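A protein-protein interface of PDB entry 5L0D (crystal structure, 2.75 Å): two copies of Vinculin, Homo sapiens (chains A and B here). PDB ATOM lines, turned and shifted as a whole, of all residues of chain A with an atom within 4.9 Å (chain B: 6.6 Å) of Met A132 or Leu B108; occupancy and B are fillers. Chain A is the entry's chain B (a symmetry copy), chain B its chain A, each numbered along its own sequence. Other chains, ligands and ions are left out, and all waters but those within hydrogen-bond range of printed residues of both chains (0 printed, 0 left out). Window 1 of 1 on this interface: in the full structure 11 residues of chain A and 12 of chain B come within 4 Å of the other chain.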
ATOM      1  N   LEU A 108      32.761   6.390  26.688  1.00  0.00           N
ATOM      2  CA  LEU A 108      32.305   6.764  25.361  1.00  0.00           C
ATOM      3  C   LEU A 108      32.525   5.668  24.356  1.00  0.00           C
ATOM      4  O   LEU A 108      31.756   5.601  23.396  1.00  0.00           O
ATOM      5  CB  LEU A 108      33.010   8.033  24.899  1.00  0.00           C
ATOM      6  CG  LEU A 108      32.754   9.273  25.726  1.00  0.00           C
ATOM      7  CD1 LEU A 108      33.774  10.333  25.391  1.00  0.00           C
ATOM      8  CD2 LEU A 108      31.304   9.743  25.595  1.00  0.00           C
ATOM      9  N   GLN A 128      26.768  12.177  17.180  1.00  0.00           N
ATOM     10  CA  GLN A 128      27.180  12.786  18.432  1.00  0.00           C
ATOM     11  C   GLN A 128      27.997  11.840  19.285  1.00  0.00           C
ATOM     12  O   GLN A 128      28.936  12.301  19.925  1.00  0.00           O
ATOM     13  CB  GLN A 128      25.991  13.312  19.197  1.00  0.00           C
ATOM     14  CG  GLN A 128      25.261  14.483  18.523  1.00  0.00           C
ATOM     15  CD  GLN A 128      26.076  15.724  18.276  1.00  0.00           C
ATOM     16  OE1 GLN A 128      26.891  16.131  19.116  1.00  0.00           O
ATOM     17  NE2 GLN A 128      25.850  16.365  17.133  1.00  0.00           N
ATOM     18  N   ALA A 129      27.701  10.521  19.262  1.00  0.00           N
ATOM     19  CA  ALA A 129      28.514   9.534  19.980  1.00  0.00           C
ATOM     20  C   ALA A 129      29.915   9.487  19.368  1.00  0.00           C
ATOM     21  O   ALA A 129      30.896   9.516  20.111  1.00  0.00           O
ATOM     22  CB  ALA A 129      27.871   8.169  19.926  1.00  0.00           C
ATOM     23  N   THR A 130      30.006   9.522  18.020  1.00  0.00           N
ATOM     24  CA  THR A 130      31.271   9.527  17.298  1.00  0.00           C
ATOM     25  C   THR A 130      32.069  10.795  17.637  1.00  0.00           C
ATOM     26  O   THR A 130      33.265  10.703  17.936  1.00  0.00           O
ATOM     27  CB  THR A 130      31.033   9.389  15.784  1.00  0.00           C
ATOM     28  OG1 THR A 130      30.420   8.125  15.499  1.00  0.00           O
ATOM     29  CG2 THR A 130      32.318   9.528  14.968  1.00  0.00           C
ATOM     30  N   GLU A 131      31.408  11.965  17.588  1.00  0.00           N
ATOM     31  CA  GLU A 131      32.022  13.274  17.842  1.00  0.00           C
ATOM     32  C   GLU A 131      32.549  13.380  19.273  1.00  0.00           C
ATOM     33  O   GLU A 131      33.628  13.937  19.474  1.00  0.00           O
ATOM     34  CB  GLU A 131      31.058  14.416  17.533  1.00  0.00           C
ATOM     35  CG  GLU A 131      30.699  14.492  16.056  1.00  0.00           C
ATOM     36  CD  GLU A 131      31.902  14.662  15.157  1.00  0.00           C
ATOM     37  OE1 GLU A 131      32.824  15.426  15.524  1.00  0.00           O
ATOM     38  OE2 GLU A 131      31.924  14.015  14.087  1.00  0.00           O
ATOM     39  N   MET A 132      31.829  12.808  20.253  1.00  0.00           N
ATOM     40  CA  MET A 132      32.295  12.801  21.630  1.00  0.00           C
ATOM     41  C   MET A 132      33.556  11.944  21.731  1.00  0.00           C
ATOM     42  O   MET A 132      34.513  12.333  22.404  1.00  0.00           O
ATOM     43  CB  MET A 132      31.218  12.284  22.577  1.00  0.00           C
ATOM     44  CG  MET A 132      30.043  13.208  22.726  1.00  0.00           C
ATOM     45  SD  MET A 132      28.694  12.410  23.638  1.00  0.00           S
ATOM     46  CE  MET A 132      29.019  13.072  25.210  1.00  0.00           C
ATOM     47  N   LEU A 133      33.578  10.794  21.029  1.00  0.00           N
ATOM     48  CA  LEU A 133      34.725   9.882  21.026  1.00  0.00           C
ATOM     49  C   LEU A 133      35.933  10.554  20.351  1.00  0.00           C
ATOM     50  O   LEU A 133      37.030  10.507  20.894  1.00  0.00           O
ATOM     51  CB  LEU A 133      34.338   8.566  20.344  1.00  0.00           C
ATOM     52  CG  LEU A 133      35.269   7.360  20.529  1.00  0.00           C
ATOM     53  CD1 LEU A 133      35.672   7.158  21.997  1.00  0.00           C
ATOM     54  CD2 LEU A 133      34.605   6.126  20.058  1.00  0.00           C
ATOM     55  N   VAL A 134      35.700  11.244  19.226  1.00  0.00           N
ATOM     56  CA  VAL A 134      36.703  12.013  18.474  1.00  0.00           C
ATOM     57  C   VAL A 134      37.346  13.105  19.381  1.00  0.00           C
ATOM     58  O   VAL A 134      38.570  13.175  19.469  1.00  0.00           O
ATOM     59  CB  VAL A 134      36.109  12.632  17.171  1.00  0.00           C
ATOM     60  CG1 VAL A 134      37.043  13.682  16.573  1.00  0.00           C
ATOM     61  CG2 VAL A 134      35.804  11.558  16.131  1.00  0.00           C
ATOM     62  N   HIS A 135      36.529  13.926  20.054  1.00  0.00           N
ATOM     63  CA  HIS A 135      37.006  15.001  20.927  1.00  0.00           C
ATOM     64  C   HIS A 135      37.843  14.438  22.084  1.00  0.00           C
ATOM     65  O   HIS A 135      38.865  15.028  22.466  1.00  0.00           O
ATOM     66  CB  HIS A 135      35.829  15.836  21.451  1.00  0.00           C
ATOM     67  CG  HIS A 135      36.221  16.992  22.326  1.00  0.00           C
ATOM     68  ND1 HIS A 135      36.919  18.098  21.819  1.00  0.00           N
ATOM     69  CD2 HIS A 135      35.971  17.202  23.641  1.00  0.00           C
ATOM     70  CE1 HIS A 135      37.071  18.925  22.842  1.00  0.00           C
ATOM     71  NE2 HIS A 135      36.522  18.429  23.960  1.00  0.00           N
ATOM     72  N   ASN A 136      37.427  13.272  22.606  1.00  0.00           N
ATOM     73  CA  ASN A 136      38.116  12.599  23.691  1.00  0.00           C
ATOM     74  C   ASN A 136      39.494  12.107  23.229  1.00  0.00           C
ATOM     75  O   ASN A 136      40.490  12.291  23.940  1.00  0.00           O
ATOM     76  CB  ASN A 136      37.262  11.454  24.211  1.00  0.00           C
ATOM     77  CG  ASN A 136      37.773  10.909  25.503  1.00  0.00           C
ATOM     78  OD1 ASN A 136      37.366  11.331  26.591  1.00  0.00           O
ATOM     79  ND2 ASN A 136      38.749  10.032  25.406  1.00  0.00           N
ATOM     80  N   LEU B  57      15.108   8.176  33.988  1.00  0.00           N
ATOM     81  CA  LEU B  57      16.279   8.972  33.628  1.00  0.00           C
ATOM     82  C   LEU B  57      16.387   9.147  32.107  1.00  0.00           C
ATOM     83  O   LEU B  57      16.645  10.264  31.632  1.00  0.00           O
ATOM     84  CB  LEU B  57      17.560   8.331  34.194  1.00  0.00           C
ATOM     85  CG  LEU B  57      18.877   9.140  34.065  1.00  0.00           C
ATOM     86  CD1 LEU B  57      18.713  10.546  34.544  1.00  0.00           C
ATOM     87  CD2 LEU B  57      19.982   8.517  34.864  1.00  0.00           C
ATOM     88  N   THR B 103      21.395  16.206  22.366  1.00  0.00           N
ATOM     89  CA  THR B 103      21.667  14.871  21.819  1.00  0.00           C
ATOM     90  C   THR B 103      22.682  14.175  22.755  1.00  0.00           C
ATOM     91  O   THR B 103      22.506  13.005  23.131  1.00  0.00           O
ATOM     92  CB  THR B 103      22.173  14.959  20.387  1.00  0.00           C
ATOM     93  OG1 THR B 103      21.155  15.511  19.562  1.00  0.00           O
ATOM     94  CG2 THR B 103      22.574  13.607  19.839  1.00  0.00           C
ATOM     95  N   GLN B 104      23.712  14.931  23.167  1.00  0.00           N
ATOM     96  CA  GLN B 104      24.724  14.478  24.107  1.00  0.00           C
ATOM     97  C   GLN B 104      24.130  14.202  25.494  1.00  0.00           C
ATOM     98  O   GLN B 104      24.619  13.312  26.182  1.00  0.00           O
ATOM     99  CB  GLN B 104      25.842  15.500  24.199  1.00  0.00           C
ATOM    100  CG  GLN B 104      26.757  15.510  22.953  1.00  0.00           C
ATOM    101  CD  GLN B 104      28.009  16.357  23.044  1.00  0.00           C
ATOM    102  OE1 GLN B 104      28.671  16.623  22.040  1.00  0.00           O
ATOM    103  NE2 GLN B 104      28.376  16.797  24.233  1.00  0.00           N
ATOM    104  N   LEU B 105      23.058  14.920  25.894  1.00  0.00           N
ATOM    105  CA  LEU B 105      22.369  14.676  27.172  1.00  0.00           C
ATOM    106  C   LEU B 105      21.705  13.305  27.149  1.00  0.00           C
ATOM    107  O   LEU B 105      21.724  12.612  28.160  1.00  0.00           O
ATOM    108  CB  LEU B 105      21.325  15.758  27.488  1.00  0.00           C
ATOM    109  CG  LEU B 105      20.565  15.645  28.811  1.00  0.00           C
ATOM    110  CD1 LEU B 105      21.436  16.056  29.971  1.00  0.00           C
ATOM    111  CD2 LEU B 105      19.286  16.480  28.767  1.00  0.00           C
ATOM    112  N   LYS B 106      21.129  12.917  26.006  1.00  0.00           N
ATOM    113  CA  LYS B 106      20.460  11.629  25.842  1.00  0.00           C
ATOM    114  C   LYS B 106      21.486  10.492  25.962  1.00  0.00           C
ATOM    115  O   LYS B 106      21.246   9.521  26.687  1.00  0.00           O
ATOM    116  CB  LYS B 106      19.700  11.561  24.511  1.00  0.00           C
ATOM    117  CG  LYS B 106      18.502  12.506  24.422  1.00  0.00           C
ATOM    118  CD  LYS B 106      17.580  12.193  23.236  1.00  0.00           C
ATOM    119  CE  LYS B 106      18.004  12.857  21.967  1.00  0.00           C
ATOM    120  NZ  LYS B 106      17.223  12.349  20.812  1.00  0.00           N
ATOM    121  N   ILE B 107      22.644  10.648  25.297  1.00  0.00           N
ATOM    122  CA  ILE B 107      23.723   9.662  25.333  1.00  0.00           C
ATOM    123  C   ILE B 107      24.230   9.463  26.768  1.00  0.00           C
ATOM    124  O   ILE B 107      24.287   8.331  27.244  1.00  0.00           O
ATOM    125  CB  ILE B 107      24.845  10.092  24.360  1.00  0.00           C
ATOM    126  CG1 ILE B 107      24.395   9.894  22.889  1.00  0.00           C
ATOM    127  CG2 ILE B 107      26.151   9.356  24.659  1.00  0.00           C
ATOM    128  CD1 ILE B 107      25.115  10.736  21.830  1.00  0.00           C
ATOM    129  N   LEU B 108      24.566  10.556  27.457  1.00  0.00           N
ATOM    130  CA  LEU B 108      25.132  10.514  28.799  1.00  0.00           C
ATOM    131  C   LEU B 108      24.113  10.086  29.856  1.00  0.00           C
ATOM    132  O   LEU B 108      24.498   9.453  30.847  1.00  0.00           O
ATOM    133  CB  LEU B 108      25.793  11.845  29.160  1.00  0.00           C
ATOM    134  CG  LEU B 108      26.946  12.269  28.240  1.00  0.00           C
ATOM    135  CD1 LEU B 108      27.394  13.691  28.546  1.00  0.00           C
ATOM    136  CD2 LEU B 108      28.112  11.268  28.286  1.00  0.00           C
ATOM    137  N   SER B 109      22.826  10.364  29.641  1.00  0.00           N
ATOM    138  CA  SER B 109      21.775   9.890  30.563  1.00  0.00           C
ATOM    139  C   SER B 109      21.593   8.383  30.450  1.00  0.00           C
ATOM    140  O   SER B 109      21.369   7.741  31.464  1.00  0.00           O
ATOM    141  CB  SER B 109      20.437  10.566  30.287  1.00  0.00           C
ATOM    142  OG  SER B 109      20.535  11.947  30.592  1.00  0.00           O
ATOM    143  N   THR B 110      21.688   7.829  29.221  1.00  0.00           N
ATOM    144  CA  THR B 110      21.585   6.397  28.954  1.00  0.00           C
ATOM    145  C   THR B 110      22.765   5.688  29.614  1.00  0.00           C
ATOM    146  O   THR B 110      22.570   4.664  30.289  1.00  0.00           O
ATOM    147  CB  THR B 110      21.515   6.160  27.450  1.00  0.00           C
ATOM    148  OG1 THR B 110      20.416   6.895  26.916  1.00  0.00           O
ATOM    149  CG2 THR B 110      21.448   4.682  27.074  1.00  0.00           C
ATOM    150  N   VAL B 111      23.976   6.265  29.461  1.00  0.00           N
ATOM    151  CA  VAL B 111      25.195   5.774  30.097  1.00  0.00           C
ATOM    152  C   VAL B 111      24.982   5.698  31.612  1.00  0.00           C
ATOM    153  O   VAL B 111      25.174   4.631  32.204  1.00  0.00           O
ATOM    154  CB  VAL B 111      26.410   6.662  29.755  1.00  0.00           C
ATOM    155  CG1 VAL B 111      27.589   6.375  30.670  1.00  0.00           C
ATOM    156  CG2 VAL B 111      26.805   6.493  28.320  1.00  0.00           C
ATOM    157  N   LYS B 112      24.596   6.828  32.232  1.00  0.00           N
ATOM    158  CA  LYS B 112      24.385   6.897  33.673  1.00  0.00           C
ATOM    159  C   LYS B 112      23.291   5.955  34.131  1.00  0.00           C
ATOM    160  O   LYS B 112      23.474   5.294  35.141  1.00  0.00           O
ATOM    161  CB  LYS B 112      24.059   8.324  34.124  1.00  0.00           C
ATOM    162  CG  LYS B 112      24.097   8.510  35.640  1.00  0.00           C
ATOM    163  CD  LYS B 112      25.506   8.249  36.241  1.00  0.00           C
ATOM    164  CE  LYS B 112      25.411   7.902  37.703  1.00  0.00           C
ATOM    165  NZ  LYS B 112      26.744   7.651  38.296  1.00  0.00           N
ATOM    166  N   ALA B 113      22.167   5.873  33.384  1.00  0.00           N
ATOM    167  CA  ALA B 113      21.020   4.989  33.677  1.00  0.00           C
ATOM    168  C   ALA B 113      21.435   3.509  33.700  1.00  0.00           C
ATOM    169  O   ALA B 113      21.011   2.779  34.597  1.00  0.00           O
ATOM    170  CB  ALA B 113      19.901   5.196  32.669  1.00  0.00           C
ATOM    171  N   MET B 115      24.238   2.185  34.478  1.00  0.00           N
ATOM    172  CA  MET B 115      25.008   2.000  35.704  1.00  0.00           C
ATOM    173  C   MET B 115      24.201   1.997  37.008  1.00  0.00           C
ATOM    174  O   MET B 115      24.500   1.231  37.924  1.00  0.00           O
ATOM    175  CB  MET B 115      26.121   3.050  35.790  1.00  0.00           C
ATOM    176  CG  MET B 115      27.203   2.895  34.735  1.00  0.00           C
ATOM    177  SD  MET B 115      28.535   4.095  34.925  1.00  0.00           S
ATOM    178  CE  MET B 115      27.754   5.574  34.282  1.00  0.00           C
ATOM    179  N   ALA B 129      31.017   9.363  34.721  1.00  0.00           N
ATOM    180  CA  ALA B 129      29.752   9.417  33.984  1.00  0.00           C
ATOM    181  C   ALA B 129      28.852  10.490  34.575  1.00  0.00           C
ATOM    182  O   ALA B 129      28.176  11.185  33.824  1.00  0.00           O
ATOM    183  CB  ALA B 129      29.043   8.069  33.998  1.00  0.00           C
ATOM    184  N   MET B 132      30.318  13.938  33.559  1.00  0.00           N
ATOM    185  CA  MET B 132      30.079  14.258  32.159  1.00  0.00           C
ATOM    186  C   MET B 132      28.650  14.755  32.011  1.00  0.00           C
ATOM    187  O   MET B 132      28.374  15.696  31.268  1.00  0.00           O
ATOM    188  CB  MET B 132      30.307  13.029  31.278  1.00  0.00           C
ATOM    189  CG  MET B 132      31.757  12.578  31.206  1.00  0.00           C
ATOM    190  SD  MET B 132      31.970  11.077  30.228  1.00  0.00           S
ATOM    191  CE  MET B 132      31.695  11.708  28.574  1.00  0.00           C
ATOM    192  N   LEU B 133      27.747  14.103  32.735  1.00  0.00           N
ATOM    193  CA  LEU B 133      26.326  14.452  32.718  1.00  0.00           C
ATOM    194  C   LEU B 133      26.133  15.842  33.320  1.00  0.00           C
ATOM    195  O   LEU B 133      25.431  16.652  32.737  1.00  0.00           O
ATOM    196  CB  LEU B 133      25.493  13.384  33.457  1.00  0.00           C
ATOM    197  CG  LEU B 133      23.970  13.411  33.302  1.00  0.00           C
ATOM    198  CD1 LEU B 133      23.552  13.544  31.864  1.00  0.00           C
ATOM    199  CD2 LEU B 133      23.341  12.159  33.884  1.00  0.00           C
ATOM    200  N   VAL B 134      26.806  16.127  34.439  1.00  0.00           N
ATOM    201  CA  VAL B 134      26.773  17.410  35.147  1.00  0.00           C
ATOM    202  C   VAL B 134      27.231  18.542  34.204  1.00  0.00           C
ATOM    203  O   VAL B 134      26.502  19.524  34.072  1.00  0.00           O
ATOM    204  CB  VAL B 134      27.613  17.376  36.457  1.00  0.00           C
ATOM    205  CG1 VAL B 134      27.849  18.767  37.024  1.00  0.00           C
ATOM    206  CG2 VAL B 134      26.951  16.505  37.506  1.00  0.00           C
ATOM    207  N   ASN B 136      27.384  18.616  30.946  1.00  0.00           N
ATOM    208  CA  ASN B 136      26.438  18.700  29.847  1.00  0.00           C
ATOM    209  C   ASN B 136      25.188  19.477  30.283  1.00  0.00           C
ATOM    210  O   ASN B 136      24.743  20.342  29.540  1.00  0.00           O
ATOM    211  CB  ASN B 136      26.078  17.299  29.364  1.00  0.00           C
ATOM    212  CG  ASN B 136      25.269  17.317  28.107  1.00  0.00           C
ATOM    213  OD1 ASN B 136      24.057  17.487  28.118  1.00  0.00           O
ATOM    214  ND2 ASN B 136      25.945  17.272  26.968  1.00  0.00           N
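OE1 of Gln A128 sits close to OE1 of Gln B104, at 3.5 Å.
Leu A108 touches Met B132, and with the chains exchanged Met A132 touches Leu B108.
6 positions are printed for both chains.
Of the 7 pairs that touch across the chains among the printed residues, 2 have their exchanged pair printed and touching as well.
Printed residues of chain A that touch a printed residue of chain B: Leu A108, Gln A128, Ala A129 and Met A132.
Of the 18 printed residues of chain B, 5 touch a printed residue of chain A.
Along chain B the printed residues that touch a printed residue of chain A span positions 103 to 132.
Among the printed residues, no Asp or Glu carboxylate lies within 4 Å of a Lys or Arg side-chain nitrogen of the other chain.
Met A132 touches just these residues of chain B: Gln B104 and Leu B108.
Leu B108 touches just one residue of chain A: Met A132 (3.7 Å).
Printed residues of chain A within 4 Å of Thr B103: Gln A128 (3.1 Å).
Of the printed residues of chain A, Ile B107 touches Gln A128 (3.8 Å) and Ala A129 (3.7 Å).
Printed residues of chain B within 4 Å of Leu A108: Met B132 (3.6 Å).
Of the printed residues of chain A, Met B132 touches Leu A108.
Ala B129 touches none of the printed residues of chain A.
Val B134 touches none of the printed residues of chain A.
The nearest residue of chain B that does not touch Met A132 is Ile B107 (4.1 Å).
The nearest printed residue of chain A that does not touch Gln B104 is Glu A131 (5.6 Å).
CD2 of Leu A108 touches CE of Met B132 (3.6 Å).
Gln A128 touches Thr B103 (CG to CG2, 3.1 Å).
CB of Gln A128 touches CD1 of Ile B107, at 3.8 Å.
N of Ala A129 touches CD1 of Ile B107, at 3.7 Å.
CG of Gln B104 touches SD of Met A132, at 3.7 Å.
Met A132 touches Leu B108 (CE to CD2, 3.7 Å).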
